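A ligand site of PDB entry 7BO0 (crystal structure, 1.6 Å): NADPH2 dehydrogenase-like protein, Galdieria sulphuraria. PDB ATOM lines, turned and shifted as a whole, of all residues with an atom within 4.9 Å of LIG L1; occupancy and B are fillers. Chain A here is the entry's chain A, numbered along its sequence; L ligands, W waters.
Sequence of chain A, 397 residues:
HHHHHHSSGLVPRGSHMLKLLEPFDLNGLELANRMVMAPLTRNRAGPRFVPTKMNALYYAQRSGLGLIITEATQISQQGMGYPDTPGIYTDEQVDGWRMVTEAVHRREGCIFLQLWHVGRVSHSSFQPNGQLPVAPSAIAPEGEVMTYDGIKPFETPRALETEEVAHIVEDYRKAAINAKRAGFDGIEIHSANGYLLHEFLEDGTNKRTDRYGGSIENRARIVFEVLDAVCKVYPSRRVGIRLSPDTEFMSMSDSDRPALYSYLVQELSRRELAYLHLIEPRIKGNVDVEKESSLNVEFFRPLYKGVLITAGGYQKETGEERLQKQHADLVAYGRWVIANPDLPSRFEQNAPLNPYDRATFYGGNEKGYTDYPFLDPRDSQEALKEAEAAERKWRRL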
ATOM      1  N   ALA A  38     -12.001   5.350  -9.411  1.00  0.00           N
ATOM      2  CA  ALA A  38     -12.418   4.556 -10.555  1.00  0.00           C
ATOM      3  C   ALA A  38     -12.080   5.289 -11.860  1.00  0.00           C
ATOM      4  O   ALA A  38     -12.001   6.523 -11.886  1.00  0.00           O
ATOM      5  CB  ALA A  38     -13.909   4.243 -10.454  1.00  0.00           C
ATOM      6  N   PRO A  39     -11.873   4.539 -12.956  1.00  0.00           N
ATOM      7  CA  PRO A  39     -11.614   5.187 -14.258  1.00  0.00           C
ATOM      8  C   PRO A  39     -12.835   5.921 -14.754  1.00  0.00           C
ATOM      9  O   PRO A  39     -13.930   5.353 -14.792  1.00  0.00           O
ATOM     10  CB  PRO A  39     -11.271   4.010 -15.179  1.00  0.00           C
ATOM     11  CG  PRO A  39     -11.916   2.792 -14.555  1.00  0.00           C
ATOM     12  CD  PRO A  39     -11.920   3.068 -13.043  1.00  0.00           C
ATOM     13  N   LEU A  40     -12.639   7.144 -15.233  1.00  0.00           N
ATOM     14  CA  LEU A  40     -13.788   8.011 -15.571  1.00  0.00           C
ATOM     15  C   LEU A  40     -13.482   8.811 -16.832  1.00  0.00           C
ATOM     16  O   LEU A  40     -12.707   9.777 -16.818  1.00  0.00           O
ATOM     17  CB  LEU A  40     -14.100   8.904 -14.369  1.00  0.00           C
ATOM     18  CG  LEU A  40     -14.594   8.281 -13.041  1.00  0.00           C
ATOM     19  CD1 LEU A  40     -14.530   9.391 -12.000  1.00  0.00           C
ATOM     20  CD2 LEU A  40     -16.039   7.779 -13.000  1.00  0.00           C
ATOM     21  N   THR A  41     -14.123   8.448 -17.926  1.00  0.00           N
ATOM     22  CA  THR A  41     -14.056   9.245 -19.148  1.00  0.00           C
ATOM     23  C   THR A  41     -14.627  10.639 -18.881  1.00  0.00           C
ATOM     24  O   THR A  41     -15.735  10.765 -18.366  1.00  0.00           O
ATOM     25  CB  THR A  41     -14.870   8.557 -20.230  1.00  0.00           C
ATOM     26  OG1 THR A  41     -14.242   7.314 -20.559  1.00  0.00           O
ATOM     27  CG2 THR A  41     -14.916   9.440 -21.474  1.00  0.00           C
ATOM     28  N   GLU A  71      -8.999   7.783 -16.635  1.00  0.00           N
ATOM     29  CA  GLU A  71     -10.040   7.624 -17.656  1.00  0.00           C
ATOM     30  C   GLU A  71      -9.515   6.685 -18.744  1.00  0.00           C
ATOM     31  O   GLU A  71      -8.319   6.571 -18.924  1.00  0.00           O
ATOM     32  CB  GLU A  71     -10.210   8.971 -18.315  1.00  0.00           C
ATOM     33  CG  GLU A  71      -8.938   9.495 -18.945  1.00  0.00           C
ATOM     34  CD  GLU A  71      -8.953  10.999 -19.095  1.00  0.00           C
ATOM     35  OE1 GLU A  71      -9.760  11.492 -19.843  1.00  0.00           O
ATOM     36  OE2 GLU A  71      -8.210  11.643 -18.404  1.00  0.00           O
ATOM     37  N   ALA A  72     -10.443   6.033 -19.419  1.00  0.00           N
ATOM     38  CA  ALA A  72     -10.040   5.140 -20.497  1.00  0.00           C
ATOM     39  C   ALA A  72      -9.200   5.920 -21.510  1.00  0.00           C
ATOM     40  O   ALA A  72      -9.517   7.029 -21.841  1.00  0.00           O
ATOM     41  CB  ALA A  72     -11.257   4.477 -21.060  1.00  0.00           C
ATOM     42  N   GLN A 114      -5.500   3.279 -17.760  1.00  0.00           N
ATOM     43  CA  GLN A 114      -6.438   2.287 -18.286  1.00  0.00           C
ATOM     44  C   GLN A 114      -6.384   2.298 -19.808  1.00  0.00           C
ATOM     45  O   GLN A 114      -6.708   3.312 -20.433  1.00  0.00           O
ATOM     46  CB  GLN A 114      -7.874   2.585 -17.837  1.00  0.00           C
ATOM     47  CG  GLN A 114      -8.805   1.459 -18.258  1.00  0.00           C
ATOM     48  CD  GLN A 114     -10.249   1.744 -17.925  1.00  0.00           C
ATOM     49  OE1 GLN A 114     -10.808   2.699 -18.429  1.00  0.00           O
ATOM     50  NE2 GLN A 114     -10.859   0.887 -17.093  1.00  0.00           N
ATOM     51  N   HIS A 190      -8.730  -2.448 -20.030  1.00  0.00           N
ATOM     52  CA  HIS A 190     -10.180  -2.278 -19.959  1.00  0.00           C
ATOM     53  C   HIS A 190     -10.786  -3.516 -20.624  1.00  0.00           C
ATOM     54  O   HIS A 190     -10.651  -3.718 -21.852  1.00  0.00           O
ATOM     55  CB  HIS A 190     -10.654  -1.034 -20.697  1.00  0.00           C
ATOM     56  CG  HIS A 190     -12.053  -0.600 -20.309  1.00  0.00           C
ATOM     57  ND1 HIS A 190     -13.179  -1.243 -20.757  1.00  0.00           N
ATOM     58  CD2 HIS A 190     -12.477   0.556 -19.754  1.00  0.00           C
ATOM     59  CE1 HIS A 190     -14.249  -0.597 -20.323  1.00  0.00           C
ATOM     60  NE2 HIS A 190     -13.860   0.512 -19.747  1.00  0.00           N
ATOM     61  N   ASN A 193     -17.655  -3.382 -19.954  1.00  0.00           N
ATOM     62  CA  ASN A 193     -18.561  -2.333 -20.415  1.00  0.00           C
ATOM     63  C   ASN A 193     -18.742  -2.277 -21.921  1.00  0.00           C
ATOM     64  O   ASN A 193     -19.019  -1.215 -22.489  1.00  0.00           O
ATOM     65  CB  ASN A 193     -18.118  -0.974 -19.866  1.00  0.00           C
ATOM     66  CG  ASN A 193     -18.328  -0.894 -18.370  1.00  0.00           C
ATOM     67  OD1 ASN A 193     -19.014  -1.741 -17.783  1.00  0.00           O
ATOM     68  ND2 ASN A 193     -17.710   0.090 -17.737  1.00  0.00           N
ATOM     69  N   ARG A 242      -9.855  -5.072 -15.709  1.00  0.00           N
ATOM     70  CA  ARG A 242     -11.198  -4.706 -15.258  1.00  0.00           C
ATOM     71  C   ARG A 242     -12.254  -5.490 -16.031  1.00  0.00           C
ATOM     72  O   ARG A 242     -12.193  -5.576 -17.261  1.00  0.00           O
ATOM     73  CB  ARG A 242     -11.456  -3.209 -15.422  1.00  0.00           C
ATOM     74  CG  ARG A 242     -12.682  -2.731 -14.656  1.00  0.00           C
ATOM     75  CD  ARG A 242     -12.803  -1.213 -14.661  1.00  0.00           C
ATOM     76  NE  ARG A 242     -13.455  -0.791 -13.438  1.00  0.00           N
ATOM     77  CZ  ARG A 242     -14.379   0.154 -13.338  1.00  0.00           C
ATOM     78  NH1 ARG A 242     -14.823   0.842 -14.381  1.00  0.00           N
ATOM     79  NH2 ARG A 242     -14.887   0.381 -12.162  1.00  0.00           N
ATOM     80  N   ILE A 279     -16.690  -4.737 -11.581  1.00  0.00           N
ATOM     81  CA  ILE A 279     -17.807  -3.792 -11.545  1.00  0.00           C
ATOM     82  C   ILE A 279     -19.056  -4.546 -11.086  1.00  0.00           C
ATOM     83  O   ILE A 279     -19.362  -5.626 -11.605  1.00  0.00           O
ATOM     84  CB  ILE A 279     -18.032  -3.158 -12.934  1.00  0.00           C
ATOM     85  CG1 ILE A 279     -16.729  -2.577 -13.485  1.00  0.00           C
ATOM     86  CG2 ILE A 279     -19.103  -2.084 -12.856  1.00  0.00           C
ATOM     87  CD1 ILE A 279     -16.915  -1.830 -14.800  1.00  0.00           C
ATOM     88  N   ILE A 283     -24.520  -1.610 -11.657  1.00  0.00           N
ATOM     89  CA  ILE A 283     -24.105  -0.482 -12.486  1.00  0.00           C
ATOM     90  C   ILE A 283     -24.255  -0.878 -13.950  1.00  0.00           C
ATOM     91  O   ILE A 283     -23.850  -1.985 -14.353  1.00  0.00           O
ATOM     92  CB  ILE A 283     -22.654  -0.057 -12.200  1.00  0.00           C
ATOM     93  CG1 ILE A 283     -22.493   0.443 -10.766  1.00  0.00           C
ATOM     94  CG2 ILE A 283     -22.247   1.015 -13.216  1.00  0.00           C
ATOM     95  CD1 ILE A 283     -23.270   1.705 -10.431  1.00  0.00           C
ATOM     96  N   GLY A 285     -22.818   0.659 -16.897  1.00  0.00           N
ATOM     97  CA  GLY A 285     -21.869   1.574 -17.502  1.00  0.00           C
ATOM     98  C   GLY A 285     -21.573   2.804 -16.676  1.00  0.00           C
ATOM     99  O   GLY A 285     -20.522   2.899 -16.035  1.00  0.00           O
ATOM    100  N   ASN A 286     -22.505   3.756 -16.657  1.00  0.00           N
ATOM    101  CA  ASN A 286     -22.295   5.039 -15.991  1.00  0.00           C
ATOM    102  C   ASN A 286     -23.509   5.495 -15.208  1.00  0.00           C
ATOM    103  O   ASN A 286     -23.584   6.670 -14.806  1.00  0.00           O
ATOM    104  CB  ASN A 286     -21.896   6.094 -17.020  1.00  0.00           C
ATOM    105  CG  ASN A 286     -22.920   6.248 -18.145  1.00  0.00           C
ATOM    106  OD1 ASN A 286     -23.947   5.573 -18.151  1.00  0.00           O
ATOM    107  ND2 ASN A 286     -22.657   7.176 -19.058  1.00  0.00           N
ATOM    108  N   ASP A 288     -26.921   3.931 -12.452  1.00  0.00           N
ATOM    109  CA  ASP A 288     -27.351   2.775 -11.640  1.00  0.00           C
ATOM    110  C   ASP A 288     -28.515   2.042 -12.296  1.00  0.00           C
ATOM    111  O   ASP A 288     -29.300   2.619 -13.033  1.00  0.00           O
ATOM    112  CB  ASP A 288     -27.709   3.196 -10.219  1.00  0.00           C
ATOM    113  CG  ASP A 288     -26.554   3.740  -9.461  1.00  0.00           C
ATOM    114  OD1 ASP A 288     -25.411   3.422  -9.816  1.00  0.00           O
ATOM    115  OD2 ASP A 288     -26.788   4.505  -8.513  1.00  0.00           O
ATOM    116  N   ALA A 311     -16.091  -2.333  -7.419  1.00  0.00           N
ATOM    117  CA  ALA A 311     -16.533  -1.029  -7.876  1.00  0.00           C
ATOM    118  C   ALA A 311     -18.022  -1.035  -8.200  1.00  0.00           C
ATOM    119  O   ALA A 311     -18.580  -2.060  -8.614  1.00  0.00           O
ATOM    120  CB  ALA A 311     -15.763  -0.572  -9.129  1.00  0.00           C
ATOM    121  N   GLY A 312     -18.656   0.113  -8.018  1.00  0.00           N
ATOM    122  CA  GLY A 312     -19.999   0.339  -8.531  1.00  0.00           C
ATOM    123  C   GLY A 312     -21.101   0.387  -7.496  1.00  0.00           C
ATOM    124  O   GLY A 312     -21.442  -0.643  -6.889  1.00  0.00           O
ATOM    125  N   GLY A 313     -21.629   1.586  -7.262  1.00  0.00           N
ATOM    126  CA  GLY A 313     -22.716   1.811  -6.325  1.00  0.00           C
ATOM    127  C   GLY A 313     -22.336   1.978  -4.870  1.00  0.00           C
ATOM    128  O   GLY A 313     -23.239   2.104  -4.023  1.00  0.00           O
ATOM    129  N   TYR A 314     -21.053   2.002  -4.526  1.00  0.00           N
ATOM    130  CA  TYR A 314     -20.715   2.028  -3.109  1.00  0.00           C
ATOM    131  C   TYR A 314     -20.846   3.415  -2.485  1.00  0.00           C
ATOM    132  O   TYR A 314     -20.726   4.455  -3.143  1.00  0.00           O
ATOM    133  CB  TYR A 314     -19.307   1.478  -2.846  1.00  0.00           C
ATOM    134  CG  TYR A 314     -19.202  -0.004  -3.137  1.00  0.00           C
ATOM    135  CD1 TYR A 314     -19.738  -0.934  -2.256  1.00  0.00           C
ATOM    136  CD2 TYR A 314     -18.573  -0.492  -4.278  1.00  0.00           C
ATOM    137  CE1 TYR A 314     -19.668  -2.290  -2.494  1.00  0.00           C
ATOM    138  CE2 TYR A 314     -18.498  -1.860  -4.535  1.00  0.00           C
ATOM    139  CZ  TYR A 314     -19.044  -2.745  -3.627  1.00  0.00           C
ATOM    140  OH  TYR A 314     -18.991  -4.111  -3.856  1.00  0.00           O
ATOM    141  N   ALA A 332     -13.396   0.963  -5.156  1.00  0.00           N
ATOM    142  CA  ALA A 332     -13.279   2.023  -6.150  1.00  0.00           C
ATOM    143  C   ALA A 332     -14.543   2.862  -6.142  1.00  0.00           C
ATOM    144  O   ALA A 332     -15.647   2.320  -6.145  1.00  0.00           O
ATOM    145  CB  ALA A 332     -13.069   1.452  -7.566  1.00  0.00           C
ATOM    146  N   TYR A 333     -14.364   4.176  -6.139  1.00  0.00           N
ATOM    147  CA  TYR A 333     -15.452   5.134  -6.184  1.00  0.00           C
ATOM    148  C   TYR A 333     -15.273   5.993  -7.417  1.00  0.00           C
ATOM    149  O   TYR A 333     -14.201   6.583  -7.620  1.00  0.00           O
ATOM    150  CB  TYR A 333     -15.474   6.016  -4.936  1.00  0.00           C
ATOM    151  CG  TYR A 333     -15.821   5.289  -3.654  1.00  0.00           C
ATOM    152  CD1 TYR A 333     -14.848   4.600  -2.958  1.00  0.00           C
ATOM    153  CD2 TYR A 333     -17.113   5.263  -3.171  1.00  0.00           C
ATOM    154  CE1 TYR A 333     -15.131   3.927  -1.763  1.00  0.00           C
ATOM    155  CE2 TYR A 333     -17.414   4.579  -1.988  1.00  0.00           C
ATOM    156  CZ  TYR A 333     -16.425   3.918  -1.297  1.00  0.00           C
ATOM    157  OH  TYR A 333     -16.729   3.250  -0.133  1.00  0.00           O
ATOM    158  N   GLY A 334     -16.316   6.021  -8.275  1.00  0.00           N
ATOM    159  CA  GLY A 334     -16.363   6.859  -9.465  1.00  0.00           C
ATOM    160  C   GLY A 334     -17.036   8.211  -9.231  1.00  0.00           C
ATOM    161  O   GLY A 334     -16.344   9.211  -8.997  1.00  0.00           O
ATOM    162  N   ARG A 335     -18.372   8.277  -9.299  1.00  0.00           N
ATOM    163  CA  ARG A 335     -19.040   9.575  -9.279  1.00  0.00           C
ATOM    164  C   ARG A 335     -18.771  10.389  -8.017  1.00  0.00           C
ATOM    165  O   ARG A 335     -18.670  11.621  -8.069  1.00  0.00           O
ATOM    166  CB  ARG A 335     -20.549   9.381  -9.443  1.00  0.00           C
ATOM    167  CG  ARG A 335     -20.912   8.883 -10.839  1.00  0.00           C
ATOM    168  CD  ARG A 335     -22.262   8.221 -10.917  1.00  0.00           C
ATOM    169  NE  ARG A 335     -22.357   6.971 -10.202  1.00  0.00           N
ATOM    170  CZ  ARG A 335     -23.493   6.346  -9.944  1.00  0.00           C
ATOM    171  NH1 ARG A 335     -23.475   5.202  -9.272  1.00  0.00           N
ATOM    172  NH2 ARG A 335     -24.656   6.847 -10.392  1.00  0.00           N
ATOM    173  N   ILE A 338     -15.579  12.177  -8.618  1.00  0.00           N
ATOM    174  CA  ILE A 338     -15.748  13.358  -9.449  1.00  0.00           C
ATOM    175  C   ILE A 338     -16.003  14.573  -8.579  1.00  0.00           C
ATOM    176  O   ILE A 338     -15.416  15.634  -8.765  1.00  0.00           O
ATOM    177  CB  ILE A 338     -16.893  13.173 -10.476  1.00  0.00           C
ATOM    178  CG1 ILE A 338     -16.538  12.063 -11.488  1.00  0.00           C
ATOM    179  CG2 ILE A 338     -17.178  14.498 -11.210  1.00  0.00           C
ATOM    180  CD1 ILE A 338     -17.549  11.834 -12.642  1.00  0.00           C
ATOM    181  N   PHE A 361     -20.288  15.793 -16.394  1.00  0.00           N
ATOM    182  CA  PHE A 361     -19.412  14.630 -16.495  1.00  0.00           C
ATOM    183  C   PHE A 361     -18.605  14.647 -17.790  1.00  0.00           C
ATOM    184  O   PHE A 361     -17.416  14.328 -17.784  1.00  0.00           O
ATOM    185  CB  PHE A 361     -20.211  13.340 -16.409  1.00  0.00           C
ATOM    186  CG  PHE A 361     -20.693  12.996 -15.011  1.00  0.00           C
ATOM    187  CD1 PHE A 361     -20.354  13.793 -13.928  1.00  0.00           C
ATOM    188  CD2 PHE A 361     -21.448  11.852 -14.789  1.00  0.00           C
ATOM    189  CE1 PHE A 361     -20.796  13.481 -12.655  1.00  0.00           C
ATOM    190  CE2 PHE A 361     -21.884  11.511 -13.516  1.00  0.00           C
ATOM    191  CZ  PHE A 361     -21.547  12.325 -12.452  1.00  0.00           C
ATOM    192  N   TYR A 362     -19.247  14.941 -18.918  1.00  0.00           N
ATOM    193  CA  TYR A 362     -18.623  14.680 -20.219  1.00  0.00           C
ATOM    194  C   TYR A 362     -18.429  15.967 -20.999  1.00  0.00           C
ATOM    195  O   TYR A 362     -19.404  16.692 -21.270  1.00  0.00           O
ATOM    196  CB  TYR A 362     -19.426  13.689 -21.051  1.00  0.00           C
ATOM    197  CG  TYR A 362     -19.814  12.423 -20.345  1.00  0.00           C
ATOM    198  CD1 TYR A 362     -18.856  11.453 -20.070  1.00  0.00           C
ATOM    199  CD2 TYR A 362     -21.129  12.163 -19.997  1.00  0.00           C
ATOM    200  CE1 TYR A 362     -19.185  10.275 -19.443  1.00  0.00           C
ATOM    201  CE2 TYR A 362     -21.484  10.978 -19.360  1.00  0.00           C
ATOM    202  CZ  TYR A 362     -20.511  10.036 -19.089  1.00  0.00           C
ATOM    203  OH  TYR A 362     -20.832   8.853 -18.484  1.00  0.00           O
HETATM  204  N1  LIG L   1     -15.413   2.902 -16.405  1.00  0.00           N
HETATM  205  C1  LIG L   1     -14.288   2.490 -17.085  1.00  0.00           C
HETATM  206  O1  LIG L   1     -13.898   1.348 -16.938  1.00  0.00           O
HETATM  207  N2  LIG L   1     -13.632   3.347 -17.918  1.00  0.00           N
HETATM  208  C2  LIG L   1     -14.065   4.643 -18.080  1.00  0.00           C
HETATM  209  O2  LIG L   1     -13.463   5.440 -18.804  1.00  0.00           O
HETATM  210  C3  LIG L   1     -15.190   5.055 -17.378  1.00  0.00           C
HETATM  211  N3  LIG L   1     -15.663   6.338 -17.513  1.00  0.00           N
HETATM  212  C4  LIG L   1     -16.755   6.749 -16.784  1.00  0.00           C
HETATM  213  C5  LIG L   1     -17.217   8.052 -16.875  1.00  0.00           C
HETATM  214  C6  LIG L   1     -18.341   8.444 -16.141  1.00  0.00           C
HETATM  215  C7  LIG L   1     -18.858   9.837 -16.237  1.00  0.00           C
HETATM  216  C8  LIG L   1     -18.970   7.531 -15.313  1.00  0.00           C
HETATM  217  C9  LIG L   1     -20.184   7.903 -14.479  1.00  0.00           C
HETATM  218  C10 LIG L   1     -18.497   6.248 -15.222  1.00  0.00           C
HETATM  219  C11 LIG L   1     -17.384   5.857 -15.943  1.00  0.00           C
HETATM  220  N4  LIG L   1     -16.941   4.559 -15.838  1.00  0.00           N
HETATM  221  C12 LIG L   1     -15.836   4.173 -16.536  1.00  0.00           C
HETATM  222  C13 LIG L   1     -17.567   3.546 -14.919  1.00  0.00           C
HETATM  223  C14 LIG L   1     -16.982   3.885 -13.550  1.00  0.00           C
HETATM  224  O3  LIG L   1     -15.601   3.521 -13.514  1.00  0.00           O
HETATM  225  C15 LIG L   1     -17.712   3.247 -12.371  1.00  0.00           C
HETATM  226  O4  LIG L   1     -17.742   1.851 -12.509  1.00  0.00           O
HETATM  227  C16 LIG L   1     -19.132   3.772 -12.280  1.00  0.00           C
HETATM  228  O5  LIG L   1     -19.151   5.182 -12.226  1.00  0.00           O
HETATM  229  C17 LIG L   1     -19.813   3.160 -11.057  1.00  0.00           C
HETATM  230  O6  LIG L   1     -19.039   3.434  -9.909  1.00  0.00           O
HETATM  231  P1  LIG L   1     -19.634   4.540  -8.903  1.00  0.00           P
HETATM  232  O7  LIG L   1     -18.638   4.740  -7.766  1.00  0.00           O
HETATM  233  O8  LIG L   1     -19.779   5.830  -9.656  1.00  0.00           O
HETATM  234  O9  LIG L   1     -20.966   4.055  -8.367  1.00  0.00           O
HETATM  235  C1  LG2 L   2     -18.197   3.412 -19.998  1.00  0.00           C
HETATM  236  C2  LG2 L   2     -16.897   5.013 -21.201  1.00  0.00           C
HETATM  237  C3  LG2 L   2     -18.283   4.620 -20.795  1.00  0.00           C
HETATM  238  C4  LG2 L   2     -16.726   3.088 -19.879  1.00  0.00           C
HETATM  239  C5  LG2 L   2     -16.535   6.213 -22.062  1.00  0.00           C
HETATM  240  O1  LG2 L   2     -15.968   4.071 -20.626  1.00  0.00           O
HETATM  241  O2  LG2 L   2     -16.262   2.165 -19.320  1.00  0.00           O
HETATM  242  O   HOH W   1     -18.572   2.742  -6.147  1.00  0.00           O
HETATM  243  O   HOH W   2     -21.347   5.293  -5.725  1.00  0.00           O
HETATM  244  O   HOH W   3     -19.249   0.831 -14.789  1.00  0.00           O
HETATM  245  O   HOH W   4     -18.911   6.787  -6.181  1.00  0.00           O
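Water W4 lies within hydrogen-bond range of O7 of LIG L1 (2.6 Å), N of Gly 334 (3.4 Å) and N of Arg 335 (3.5 Å).
Water W3 lies within hydrogen-bond range of O of Gly 285 (2.7 Å), O4 of LIG L1 (2.9 Å) and ND2 of Asn 193 (3.4 Å).
Water W2 lies within hydrogen-bond range of the backbone carbonyl oxygen of Tyr 314 (2.8 Å) and an oxygen (O9) of LIG L1 (2.9 Å).
N3 of LIG L1 sits at hydrogen-bond distance from N of Thr 41, at 2.6 Å.
The side-chain hydroxyl of Thr 41 sits at hydrogen-bond distance from an oxygen (O2) of LIG L1 (2.7 Å).
The backbone NH (N) of Gly 334 is in hydrogen-bond range of an oxygen (O7) of LIG L1, 2.7 Å away.
An oxygen (O1) of LIG L1 sits at hydrogen-bond distance from the guanidinium group (NH1) of Arg 242, at 2.8 Å.
An oxygen (O9) of LIG L1 lies within hydrogen-bond range of the backbone NH (N) of Gly 313, 2.8 Å away.
O3 of LIG L1 is in hydrogen-bond range of O of Pro 39.
The backbone NH (N) of Arg 335 lies within hydrogen-bond range of an oxygen (O8) of LIG L1 (2.8 Å).
The guanidinium group (NE) of Arg 335 is in salt-bridge range of an oxygen (O8) of LIG L1, 2.9 Å away.
A ring nitrogen (NE2) of His 190 is in hydrogen-bond range of an oxygen (O1) of LIG L1 (2.9 Å).
The side-chain amide oxygen (OE1) of Gln 114 is in hydrogen-bond range of a nitrogen (N2) of LIG L1, at 2.9 Å.
The backbone NH (N) of Ala 72 sits at hydrogen-bond distance from an oxygen (O2) of LIG L1 (3.1 Å).
A ring nitrogen (NE2) of His 190 is in hydrogen-bond range of an oxygen (O2) of LG2 L2 (2.9 Å).
ND2 of Asn 193 is in hydrogen-bond range of O2 of LG2 L2.
The guanidinium group of Arg 335 is in salt-bridge range of the side-chain carboxylate of Asp 288 (2.7 Å).
OE1 of Gln 114 sits close to N of Ala 72 (3.5 Å).
The side-chain hydroxyl (OH) of Tyr 362 lies within hydrogen-bond range of the side-chain amide nitrogen (ND2) of Asn 286, at 2.5 Å.
The backbone NH of Ala 38 sits at hydrogen-bond distance from the backbone carbonyl oxygen of Tyr 333 (3.1 Å).
Merely in contact with LIG L1: Ala 38, Leu 40, Asn 193, Ile 283, Gly 285, Asn 286, Gly 312, Tyr 333, Phe 361 and Tyr 362.
19 residues have an atom within 4 Å of LIG L1: Ala 38, Pro 39, Leu 40, Thr 41, Ala 72, Gln 114, His 190, Asn 193, Arg 242, Ile 283, Gly 285, Asn 286, Gly 312, Gly 313, Tyr 333, Gly 334, Arg 335, Phe 361 and Tyr 362.
The nearest printed residue that does not touch LIG L1 is Glu 71 (4.1 Å).
N2 of LIG L1 sits close to O2 of LG2 L2, 3.2 Å away.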
